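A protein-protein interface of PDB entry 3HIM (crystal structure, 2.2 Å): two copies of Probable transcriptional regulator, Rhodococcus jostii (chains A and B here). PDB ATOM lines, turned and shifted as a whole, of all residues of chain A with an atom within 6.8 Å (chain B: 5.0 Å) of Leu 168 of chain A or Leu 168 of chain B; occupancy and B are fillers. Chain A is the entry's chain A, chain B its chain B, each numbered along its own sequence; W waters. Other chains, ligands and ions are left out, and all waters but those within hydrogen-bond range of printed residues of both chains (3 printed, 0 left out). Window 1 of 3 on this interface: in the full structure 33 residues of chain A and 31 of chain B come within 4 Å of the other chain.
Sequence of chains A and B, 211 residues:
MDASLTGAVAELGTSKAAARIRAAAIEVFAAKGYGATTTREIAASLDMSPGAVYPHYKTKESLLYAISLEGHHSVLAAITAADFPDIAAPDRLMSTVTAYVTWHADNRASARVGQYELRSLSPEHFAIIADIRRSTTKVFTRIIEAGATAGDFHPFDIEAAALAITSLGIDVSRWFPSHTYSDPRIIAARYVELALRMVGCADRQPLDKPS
His 104 of chain A touches none of the printed residues of chain B.
Ile 165 of chain A touches none of the printed residues of chain B.
Printed residues of chain B within 4 Å of Ser 167 of chain A: Leu 168 (3.8 Å) and Asp 171 (2.8 Å).
Of chain B, only Ala 164, Ser 167 and Leu 168 come within 4 Å of Leu 168 of chain A.
Printed residues of chain B within 4 Å of Leu 194 of chain A: Ala 164 and Met 198.
Of the printed residues of chain B, Met 198 of chain A touches Met 198 (3.7 Å).
Leu 168 of chain B touches just these residues of chain A: Ala 164 (3.6 Å), Ser 167 (3.8 Å) and Leu 168 (3.9 Å).
The nearest printed residue of chain B that does not touch Leu 168 of chain A is Met 198 of chain B (5.3 Å).
The nearest printed residue of chain B that does not touch Ser 167 of chain A is Tyr 191 of chain B (4.3 Å).
Water W1 lies within hydrogen-bond range of the side-chain carboxylate (OD1) of Asp 171 of chain A (2.5 Å) and the side-chain carboxylate (OD1) of Asp 171 of chain B (2.7 Å).
Water W3 lies within hydrogen-bond range of OH of Tyr 191 of chain B, O of Leu 168 of chain B and OG of Ser 167 of chain A.
Water W2 lies within hydrogen-bond range of O of Leu 168 of chain A (2.6 Å), OH of Tyr 191 of chain A (2.6 Å), OG of Ser 167 of chain B (2.8 Å) and NE1 of Trp 175 of chain A (3.0 Å).
The side-chain hydroxyl of Ser 167 of chain A sits at hydrogen-bond distance from the side-chain carboxylate of Asp 171 of chain B (2.8 Å).
The side-chain carboxylate (OD2) of Asp 171 of chain A lies within hydrogen-bond range of the side-chain hydroxyl (OG) of Ser 167 of chain B.
Leu 163 of chain A touches Tyr 191 of chain B, and with the chains exchanged Tyr 191 of chain A touches Leu 163 of chain B.
Ala 164 of chain A touches Leu 168 of chain B, and with the chains exchanged Leu 168 of chain A touches Ala 164 of chain B.
Ser 167 of chain A touches Leu 168 of chain B, and with the chains exchanged Leu 168 of chain A touches Ser 167 of chain B.
Leu 168 of chain B touches its own counterpart, Leu 168 of chain A.
Positions printed for both chains: 163, 164, 165, 166, 167, 168, 169, 170, 171, 172, 191 and 198.
Among the printed residues, merely in contact across the chains: Leu 163 of chain A with Tyr 191 of chain B (3.7 Å), Ala 164 of chain A with Leu 168 of chain B (3.6 Å), Ser 167 of chain A with Leu 168 of chain B (3.8 Å), Leu 168 of chain A with Ala 164 of chain B (3.6 Å), Leu 168 of chain A with Ser 167 of chain B (3.7 Å), Leu 168 of chain A with Leu 168 of chain B (3.9 Å), Trp 175 of chain A with Leu 163 of chain B (3.7 Å), Tyr 191 of chain A with Leu 163 of chain B (3.5 Å), Leu 194 of chain A with Ala 164 of chain B (3.5 Å), Leu 194 of chain A with Met 198 of chain B (3.9 Å) and Met 198 of chain A with Met 198 of chain B (3.7 Å).
The side-chain hydroxyl of Thr 166 of chain A sits at hydrogen-bond distance from the backbone carbonyl oxygen of Leu 163 of chain A, at 2.6 Å.
O of Leu 163 of chain B is in hydrogen-bond range of OG1 of Thr 166 of chain B, at 2.8 Å.
Printed residues of chain A that touch a printed residue of chain B: Leu 163, Ala 164, Ser 167, Leu 168, Asp 171, Trp 175, Tyr 191, Leu 194 and Met 198.
Hydrophobic or aromatic side chains of chain A within 4 Å of the printed part of chain B: Leu 163, Ala 164, Leu 168, Trp 175, Tyr 191, Leu 194 and Met 198.
Printed residues of chain B that touch a printed residue of chain A: Leu 163, Ala 164, Ser 167, Leu 168, Asp 171, Tyr 191 and Met 198.
Among the printed residues, 13 pairs touch across the chains.
Among the printed residues, no Asp or Glu carboxylate lies within 4 Å of a Lys or Arg side-chain nitrogen of the other chain.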
ATOM      1  N   TYR A 100      27.944  22.649  32.454  1.00  0.00           N
ATOM      2  CA  TYR A 100      26.511  22.603  32.760  1.00  0.00           C
ATOM      3  C   TYR A 100      25.968  21.172  32.806  1.00  0.00           C
ATOM      4  O   TYR A 100      25.232  20.805  33.726  1.00  0.00           O
ATOM      5  CB  TYR A 100      25.735  23.406  31.734  1.00  0.00           C
ATOM      6  CG  TYR A 100      24.297  23.680  32.125  1.00  0.00           C
ATOM      7  CD1 TYR A 100      23.993  24.437  33.255  1.00  0.00           C
ATOM      8  CD2 TYR A 100      23.248  23.199  31.350  1.00  0.00           C
ATOM      9  CE1 TYR A 100      22.676  24.692  33.609  1.00  0.00           C
ATOM     10  CE2 TYR A 100      21.936  23.454  31.683  1.00  0.00           C
ATOM     11  CZ  TYR A 100      21.660  24.197  32.817  1.00  0.00           C
ATOM     12  OH  TYR A 100      20.364  24.469  33.141  1.00  0.00           O
ATOM     13  N   VAL A 101      26.361  20.371  31.823  1.00  0.00           N
ATOM     14  CA  VAL A 101      25.912  18.983  31.718  1.00  0.00           C
ATOM     15  C   VAL A 101      26.499  18.139  32.848  1.00  0.00           C
ATOM     16  O   VAL A 101      25.784  17.372  33.506  1.00  0.00           O
ATOM     17  CB  VAL A 101      26.261  18.412  30.323  1.00  0.00           C
ATOM     18  CG1 VAL A 101      26.001  16.895  30.248  1.00  0.00           C
ATOM     19  CG2 VAL A 101      25.452  19.150  29.251  1.00  0.00           C
ATOM     20  N   HIS A 104      24.981  18.728  36.313  1.00  0.00           N
ATOM     21  CA  HIS A 104      23.682  18.046  36.412  1.00  0.00           C
ATOM     22  C   HIS A 104      23.755  16.537  36.587  1.00  0.00           C
ATOM     23  O   HIS A 104      22.966  15.966  37.335  1.00  0.00           O
ATOM     24  CB  HIS A 104      22.759  18.442  35.267  1.00  0.00           C
ATOM     25  CG  HIS A 104      22.100  19.763  35.500  1.00  0.00           C
ATOM     26  ND1 HIS A 104      21.043  19.915  36.372  1.00  0.00           N
ATOM     27  CD2 HIS A 104      22.398  21.003  35.053  1.00  0.00           C
ATOM     28  CE1 HIS A 104      20.691  21.186  36.422  1.00  0.00           C
ATOM     29  NE2 HIS A 104      21.497  21.868  35.633  1.00  0.00           N
ATOM     30  N   LEU A 163      17.386  28.770  26.196  1.00  0.00           N
ATOM     31  CA  LEU A 163      16.368  27.990  26.877  1.00  0.00           C
ATOM     32  C   LEU A 163      16.547  26.490  26.612  1.00  0.00           C
ATOM     33  O   LEU A 163      16.577  25.680  27.544  1.00  0.00           O
ATOM     34  CB  LEU A 163      14.972  28.430  26.442  1.00  0.00           C
ATOM     35  CG  LEU A 163      13.907  27.357  26.727  1.00  0.00           C
ATOM     36  CD1 LEU A 163      13.620  27.228  28.252  1.00  0.00           C
ATOM     37  CD2 LEU A 163      12.649  27.659  25.970  1.00  0.00           C
ATOM     38  N   ALA A 164      16.648  26.111  25.343  1.00  0.00           N
ATOM     39  CA  ALA A 164      16.818  24.698  25.021  1.00  0.00           C
ATOM     40  C   ALA A 164      18.099  24.131  25.647  1.00  0.00           C
ATOM     41  O   ALA A 164      18.086  23.045  26.195  1.00  0.00           O
ATOM     42  CB  ALA A 164      16.791  24.477  23.531  1.00  0.00           C
ATOM     43  N   ILE A 165      19.202  24.860  25.595  1.00  0.00           N
ATOM     44  CA  ILE A 165      20.413  24.375  26.261  1.00  0.00           C
ATOM     45  C   ILE A 165      20.167  24.162  27.768  1.00  0.00           C
ATOM     46  O   ILE A 165      20.400  23.075  28.298  1.00  0.00           O
ATOM     47  CB  ILE A 165      21.600  25.310  25.998  1.00  0.00           C
ATOM     48  CG1 ILE A 165      22.026  25.161  24.542  1.00  0.00           C
ATOM     49  CG2 ILE A 165      22.749  25.007  26.951  1.00  0.00           C
ATOM     50  CD1 ILE A 165      22.789  26.328  23.990  1.00  0.00           C
ATOM     51  N   THR A 166      19.634  25.184  28.430  1.00  0.00           N
ATOM     52  CA  THR A 166      19.366  25.080  29.866  1.00  0.00           C
ATOM     53  C   THR A 166      18.442  23.912  30.191  1.00  0.00           C
ATOM     54  O   THR A 166      18.663  23.197  31.171  1.00  0.00           O
ATOM     55  CB  THR A 166      18.751  26.353  30.433  1.00  0.00           C
ATOM     56  OG1 THR A 166      17.625  26.720  29.636  1.00  0.00           O
ATOM     57  CG2 THR A 166      19.760  27.473  30.435  1.00  0.00           C
ATOM     58  N   SER A 167      17.437  23.697  29.358  1.00  0.00           N
ATOM     59  CA  SER A 167      16.467  22.656  29.602  1.00  0.00           C
ATOM     60  C   SER A 167      17.085  21.259  29.408  1.00  0.00           C
ATOM     61  O   SER A 167      16.810  20.327  30.183  1.00  0.00           O
ATOM     62  CB  SER A 167      15.255  22.879  28.689  1.00  0.00           C
ATOM     63  OG  SER A 167      14.469  21.724  28.576  1.00  0.00           O
ATOM     64  N   LEU A 168      17.922  21.117  28.386  1.00  0.00           N
ATOM     65  CA  LEU A 168      18.642  19.869  28.169  1.00  0.00           C
ATOM     66  C   LEU A 168      19.494  19.479  29.368  1.00  0.00           C
ATOM     67  O   LEU A 168      19.492  18.328  29.789  1.00  0.00           O
ATOM     68  CB  LEU A 168      19.521  19.953  26.919  1.00  0.00           C
ATOM     69  CG  LEU A 168      18.774  19.725  25.608  1.00  0.00           C
ATOM     70  CD1 LEU A 168      19.682  20.024  24.410  1.00  0.00           C
ATOM     71  CD2 LEU A 168      18.257  18.282  25.557  1.00  0.00           C
ATOM     72  N   GLY A 169      20.225  20.443  29.909  1.00  0.00           N
ATOM     73  CA  GLY A 169      21.080  20.196  31.039  1.00  0.00           C
ATOM     74  C   GLY A 169      20.282  19.795  32.266  1.00  0.00           C
ATOM     75  O   GLY A 169      20.640  18.848  32.961  1.00  0.00           O
ATOM     76  N   ILE A 170      19.191  20.510  32.524  1.00  0.00           N
ATOM     77  CA  ILE A 170      18.388  20.240  33.704  1.00  0.00           C
ATOM     78  C   ILE A 170      17.833  18.824  33.589  1.00  0.00           C
ATOM     79  O   ILE A 170      17.883  18.056  34.547  1.00  0.00           O
ATOM     80  CB  ILE A 170      17.259  21.268  33.872  1.00  0.00           C
ATOM     81  CG1 ILE A 170      17.853  22.597  34.358  1.00  0.00           C
ATOM     82  CG2 ILE A 170      16.202  20.757  34.885  1.00  0.00           C
ATOM     83  CD1 ILE A 170      16.928  23.786  34.226  1.00  0.00           C
ATOM     84  N   ASP A 171      17.354  18.474  32.396  1.00  0.00           N
ATOM     85  CA  ASP A 171      16.701  17.184  32.196  1.00  0.00           C
ATOM     86  C   ASP A 171      17.626  15.977  32.392  1.00  0.00           C
ATOM     87  O   ASP A 171      17.167  14.875  32.724  1.00  0.00           O
ATOM     88  CB  ASP A 171      15.985  17.118  30.839  1.00  0.00           C
ATOM     89  CG  ASP A 171      15.049  15.943  30.751  1.00  0.00           C
ATOM     90  OD1 ASP A 171      14.144  15.827  31.613  1.00  0.00           O
ATOM     91  OD2 ASP A 171      15.230  15.117  29.836  1.00  0.00           O
ATOM     92  N   VAL A 172      18.921  16.194  32.205  1.00  0.00           N
ATOM     93  CA  VAL A 172      19.933  15.179  32.529  1.00  0.00           C
ATOM     94  C   VAL A 172      19.734  14.616  33.957  1.00  0.00           C
ATOM     95  O   VAL A 172      19.853  13.389  34.191  1.00  0.00           O
ATOM     96  CB  VAL A 172      21.361  15.760  32.358  1.00  0.00           C
ATOM     97  CG1 VAL A 172      22.434  14.903  33.092  1.00  0.00           C
ATOM     98  CG2 VAL A 172      21.689  15.937  30.868  1.00  0.00           C
ATOM     99  N   SER A 173      19.394  15.492  34.898  1.00  0.00           N
ATOM    100  CA  SER A 173      19.222  15.072  36.281  1.00  0.00           C
ATOM    101  C   SER A 173      18.047  14.095  36.435  1.00  0.00           C
ATOM    102  O   SER A 173      18.033  13.269  37.343  1.00  0.00           O
ATOM    103  CB  SER A 173      19.080  16.290  37.193  1.00  0.00           C
ATOM    104  OG  SER A 173      20.274  17.053  37.174  1.00  0.00           O
ATOM    105  N   TRP A 175      17.048  11.768  33.840  1.00  0.00           N
ATOM    106  CA  TRP A 175      17.290  10.459  33.182  1.00  0.00           C
ATOM    107  C   TRP A 175      18.660   9.788  33.410  1.00  0.00           C
ATOM    108  O   TRP A 175      18.811   8.582  33.188  1.00  0.00           O
ATOM    109  CB  TRP A 175      16.987  10.550  31.679  1.00  0.00           C
ATOM    110  CG  TRP A 175      17.898  11.527  30.915  1.00  0.00           C
ATOM    111  CD1 TRP A 175      17.601  12.810  30.544  1.00  0.00           C
ATOM    112  CD2 TRP A 175      19.238  11.282  30.452  1.00  0.00           C
ATOM    113  NE1 TRP A 175      18.669  13.377  29.874  1.00  0.00           N
ATOM    114  CE2 TRP A 175      19.685  12.465  29.808  1.00  0.00           C
ATOM    115  CE3 TRP A 175      20.102  10.176  30.510  1.00  0.00           C
ATOM    116  CZ2 TRP A 175      20.949  12.575  29.236  1.00  0.00           C
ATOM    117  CZ3 TRP A 175      21.368  10.292  29.951  1.00  0.00           C
ATOM    118  CH2 TRP A 175      21.780  11.488  29.316  1.00  0.00           C
ATOM    119  N   TYR A 191      26.207  16.745  23.798  1.00  0.00           N
ATOM    120  CA  TYR A 191      25.332  17.900  23.957  1.00  0.00           C
ATOM    121  C   TYR A 191      26.036  19.163  23.490  1.00  0.00           C
ATOM    122  O   TYR A 191      25.392  20.079  23.004  1.00  0.00           O
ATOM    123  CB  TYR A 191      24.838  18.028  25.395  1.00  0.00           C
ATOM    124  CG  TYR A 191      23.552  17.265  25.698  1.00  0.00           C
ATOM    125  CD1 TYR A 191      22.965  16.434  24.751  1.00  0.00           C
ATOM    126  CD2 TYR A 191      22.935  17.376  26.954  1.00  0.00           C
ATOM    127  CE1 TYR A 191      21.783  15.737  25.026  1.00  0.00           C
ATOM    128  CE2 TYR A 191      21.771  16.674  27.258  1.00  0.00           C
ATOM    129  CZ  TYR A 191      21.197  15.852  26.281  1.00  0.00           C
ATOM    130  OH  TYR A 191      20.038  15.164  26.564  1.00  0.00           O
ATOM    131  N   LEU A 194      25.405  19.211  19.809  1.00  0.00           N
ATOM    132  CA  LEU A 194      24.030  19.647  19.516  1.00  0.00           C
ATOM    133  C   LEU A 194      23.829  21.148  19.695  1.00  0.00           C
ATOM    134  O   LEU A 194      23.191  21.781  18.868  1.00  0.00           O
ATOM    135  CB  LEU A 194      23.027  18.861  20.355  1.00  0.00           C
ATOM    136  CG  LEU A 194      22.969  17.384  19.957  1.00  0.00           C
ATOM    137  CD1 LEU A 194      22.099  16.583  20.940  1.00  0.00           C
ATOM    138  CD2 LEU A 194      22.479  17.212  18.485  1.00  0.00           C
ATOM    139  N   ALA A 195      24.405  21.701  20.767  1.00  0.00           N
ATOM    140  CA  ALA A 195      24.335  23.128  21.056  1.00  0.00           C
ATOM    141  C   ALA A 195      25.020  23.950  19.977  1.00  0.00           C
ATOM    142  O   ALA A 195      24.465  24.947  19.528  1.00  0.00           O
ATOM    143  CB  ALA A 195      24.955  23.425  22.409  1.00  0.00           C
ATOM    144  N   MET A 198      22.786  23.910  17.047  1.00  0.00           N
ATOM    145  CA  MET A 198      21.596  24.684  17.346  1.00  0.00           C
ATOM    146  C   MET A 198      21.784  26.138  16.935  1.00  0.00           C
ATOM    147  O   MET A 198      20.905  26.720  16.310  1.00  0.00           O
ATOM    148  CB  MET A 198      21.256  24.606  18.837  1.00  0.00           C
ATOM    149  CG  MET A 198      20.366  23.437  19.228  1.00  0.00           C
ATOM    150  SD  MET A 198      19.866  23.647  20.957  1.00  0.00           S
ATOM    151  CE  MET A 198      20.808  22.311  21.669  1.00  0.00           C
ATOM    152  N   LEU B 163      17.325  11.473  21.606  1.00  0.00           N
ATOM    153  CA  LEU B 163      17.317  11.786  23.055  1.00  0.00           C
ATOM    154  C   LEU B 163      17.086  13.274  23.299  1.00  0.00           C
ATOM    155  O   LEU B 163      16.168  13.642  24.040  1.00  0.00           O
ATOM    156  CB  LEU B 163      18.593  11.355  23.790  1.00  0.00           C
ATOM    157  CG  LEU B 163      18.824  12.033  25.180  1.00  0.00           C
ATOM    158  CD1 LEU B 163      17.799  11.562  26.273  1.00  0.00           C
ATOM    159  CD2 LEU B 163      20.236  11.825  25.704  1.00  0.00           C
ATOM    160  N   ALA B 164      17.886  14.130  22.663  1.00  0.00           N
ATOM    161  CA  ALA B 164      17.760  15.550  22.948  1.00  0.00           C
ATOM    162  C   ALA B 164      16.352  16.064  22.648  1.00  0.00           C
ATOM    163  O   ALA B 164      15.802  16.863  23.409  1.00  0.00           O
ATOM    164  CB  ALA B 164      18.811  16.360  22.220  1.00  0.00           C
ATOM    165  N   ILE B 165      15.765  15.610  21.543  1.00  0.00           N
ATOM    166  CA  ILE B 165      14.424  16.042  21.180  1.00  0.00           C
ATOM    167  C   ILE B 165      13.378  15.532  22.179  1.00  0.00           C
ATOM    168  O   ILE B 165      12.474  16.262  22.593  1.00  0.00           O
ATOM    169  CB  ILE B 165      14.067  15.622  19.721  1.00  0.00           C
ATOM    170  CG1 ILE B 165      14.806  16.508  18.712  1.00  0.00           C
ATOM    171  CG2 ILE B 165      12.554  15.696  19.490  1.00  0.00           C
ATOM    172  CD1 ILE B 165      14.951  15.868  17.325  1.00  0.00           C
ATOM    173  N   THR B 166      13.507  14.278  22.587  1.00  0.00           N
ATOM    174  CA  THR B 166      12.528  13.698  23.493  1.00  0.00           C
ATOM    175  C   THR B 166      12.691  14.390  24.854  1.00  0.00           C
ATOM    176  O   THR B 166      11.698  14.726  25.516  1.00  0.00           O
ATOM    177  CB  THR B 166      12.675  12.174  23.599  1.00  0.00           C
ATOM    178  OG1 THR B 166      13.989  11.867  24.036  1.00  0.00           O
ATOM    179  CG2 THR B 166      12.525  11.553  22.254  1.00  0.00           C
ATOM    180  N   SER B 167      13.945  14.649  25.223  1.00  0.00           N
ATOM    181  CA  SER B 167      14.252  15.350  26.454  1.00  0.00           C
ATOM    182  C   SER B 167      13.637  16.775  26.514  1.00  0.00           C
ATOM    183  O   SER B 167      13.028  17.168  27.530  1.00  0.00           O
ATOM    184  CB  SER B 167      15.763  15.368  26.681  1.00  0.00           C
ATOM    185  OG  SER B 167      16.051  16.286  27.697  1.00  0.00           O
ATOM    186  N   LEU B 168      13.770  17.535  25.422  1.00  0.00           N
ATOM    187  CA  LEU B 168      13.162  18.888  25.341  1.00  0.00           C
ATOM    188  C   LEU B 168      11.646  18.897  25.504  1.00  0.00           C
ATOM    189  O   LEU B 168      11.109  19.727  26.243  1.00  0.00           O
ATOM    190  CB  LEU B 168      13.525  19.605  24.029  1.00  0.00           C
ATOM    191  CG  LEU B 168      14.982  20.058  23.937  1.00  0.00           C
ATOM    192  CD1 LEU B 168      15.295  20.492  22.519  1.00  0.00           C
ATOM    193  CD2 LEU B 168      15.226  21.178  24.919  1.00  0.00           C
ATOM    194  N   GLY B 169      10.962  17.996  24.798  1.00  0.00           N
ATOM    195  CA  GLY B 169       9.490  17.880  24.898  1.00  0.00           C
ATOM    196  C   GLY B 169       9.051  17.541  26.327  1.00  0.00           C
ATOM    197  O   GLY B 169       8.201  18.220  26.901  1.00  0.00           O
ATOM    198  N   ILE B 170       9.669  16.515  26.910  1.00  0.00           N
ATOM    199  CA  ILE B 170       9.352  16.102  28.260  1.00  0.00           C
ATOM    200  C   ILE B 170       9.583  17.220  29.275  1.00  0.00           C
ATOM    201  O   ILE B 170       8.788  17.377  30.199  1.00  0.00           O
ATOM    202  CB  ILE B 170      10.178  14.869  28.659  1.00  0.00           C
ATOM    203  CG1 ILE B 170       9.652  13.629  27.921  1.00  0.00           C
ATOM    204  CG2 ILE B 170      10.159  14.681  30.192  1.00  0.00           C
ATOM    205  CD1 ILE B 170      10.652  12.453  27.879  1.00  0.00           C
ATOM    206  N   ASP B 171      10.651  18.005  29.101  1.00  0.00           N
ATOM    207  CA  ASP B 171      10.950  19.054  30.075  1.00  0.00           C
ATOM    208  C   ASP B 171       9.991  20.241  29.982  1.00  0.00           C
ATOM    209  O   ASP B 171       9.791  20.955  30.949  1.00  0.00           O
ATOM    210  CB  ASP B 171      12.397  19.525  29.982  1.00  0.00           C
ATOM    211  CG  ASP B 171      12.820  20.335  31.199  1.00  0.00           C
ATOM    212  OD1 ASP B 171      12.881  19.781  32.330  1.00  0.00           O
ATOM    213  OD2 ASP B 171      13.097  21.534  31.021  1.00  0.00           O
ATOM    214  N   VAL B 172       9.397  20.439  28.811  1.00  0.00           N
ATOM    215  CA  VAL B 172       8.329  21.423  28.652  1.00  0.00           C
ATOM    216  C   VAL B 172       7.261  21.203  29.728  1.00  0.00           C
ATOM    217  O   VAL B 172       6.697  22.150  30.245  1.00  0.00           O
ATOM    218  CB  VAL B 172       7.701  21.350  27.217  1.00  0.00           C
ATOM    219  CG1 VAL B 172       6.289  21.999  27.152  1.00  0.00           C
ATOM    220  CG2 VAL B 172       8.659  21.944  26.145  1.00  0.00           C
ATOM    221  N   TYR B 191      11.202  25.121  18.848  1.00  0.00           N
ATOM    222  CA  TYR B 191      11.860  23.841  19.041  1.00  0.00           C
ATOM    223  C   TYR B 191      11.970  23.105  17.729  1.00  0.00           C
ATOM    224  O   TYR B 191      12.920  22.353  17.514  1.00  0.00           O
ATOM    225  CB  TYR B 191      11.126  23.009  20.085  1.00  0.00           C
ATOM    226  CG  TYR B 191      11.555  23.312  21.498  1.00  0.00           C
ATOM    227  CD1 TYR B 191      12.348  24.430  21.805  1.00  0.00           C
ATOM    228  CD2 TYR B 191      11.152  22.489  22.544  1.00  0.00           C
ATOM    229  CE1 TYR B 191      12.746  24.687  23.122  1.00  0.00           C
ATOM    230  CE2 TYR B 191      11.524  22.739  23.846  1.00  0.00           C
ATOM    231  CZ  TYR B 191      12.315  23.825  24.146  1.00  0.00           C
ATOM    232  OH  TYR B 191      12.670  24.022  25.481  1.00  0.00           O
ATOM    233  N   MET B 198      19.778  20.826  14.821  1.00  0.00           N
ATOM    234  CA  MET B 198      20.432  19.735  15.515  1.00  0.00           C
ATOM    235  C   MET B 198      20.770  18.588  14.561  1.00  0.00           C
ATOM    236  O   MET B 198      21.865  18.023  14.637  1.00  0.00           O
ATOM    237  CB  MET B 198      19.538  19.213  16.649  1.00  0.00           C
ATOM    238  CG  MET B 198      19.714  19.970  17.966  1.00  0.00           C
ATOM    239  SD  MET B 198      18.715  19.221  19.280  1.00  0.00           S
ATOM    240  CE  MET B 198      17.253  20.245  19.111  1.00  0.00           C
HETATM  241  O   HOH W   1      12.420  17.160  32.821  1.00  0.00           O
HETATM  242  O   HOH W   2      18.703  16.101  28.646  1.00  0.00           O
HETATM  243  O   HOH W   3      12.176  22.023  27.092  1.00  0.00           O
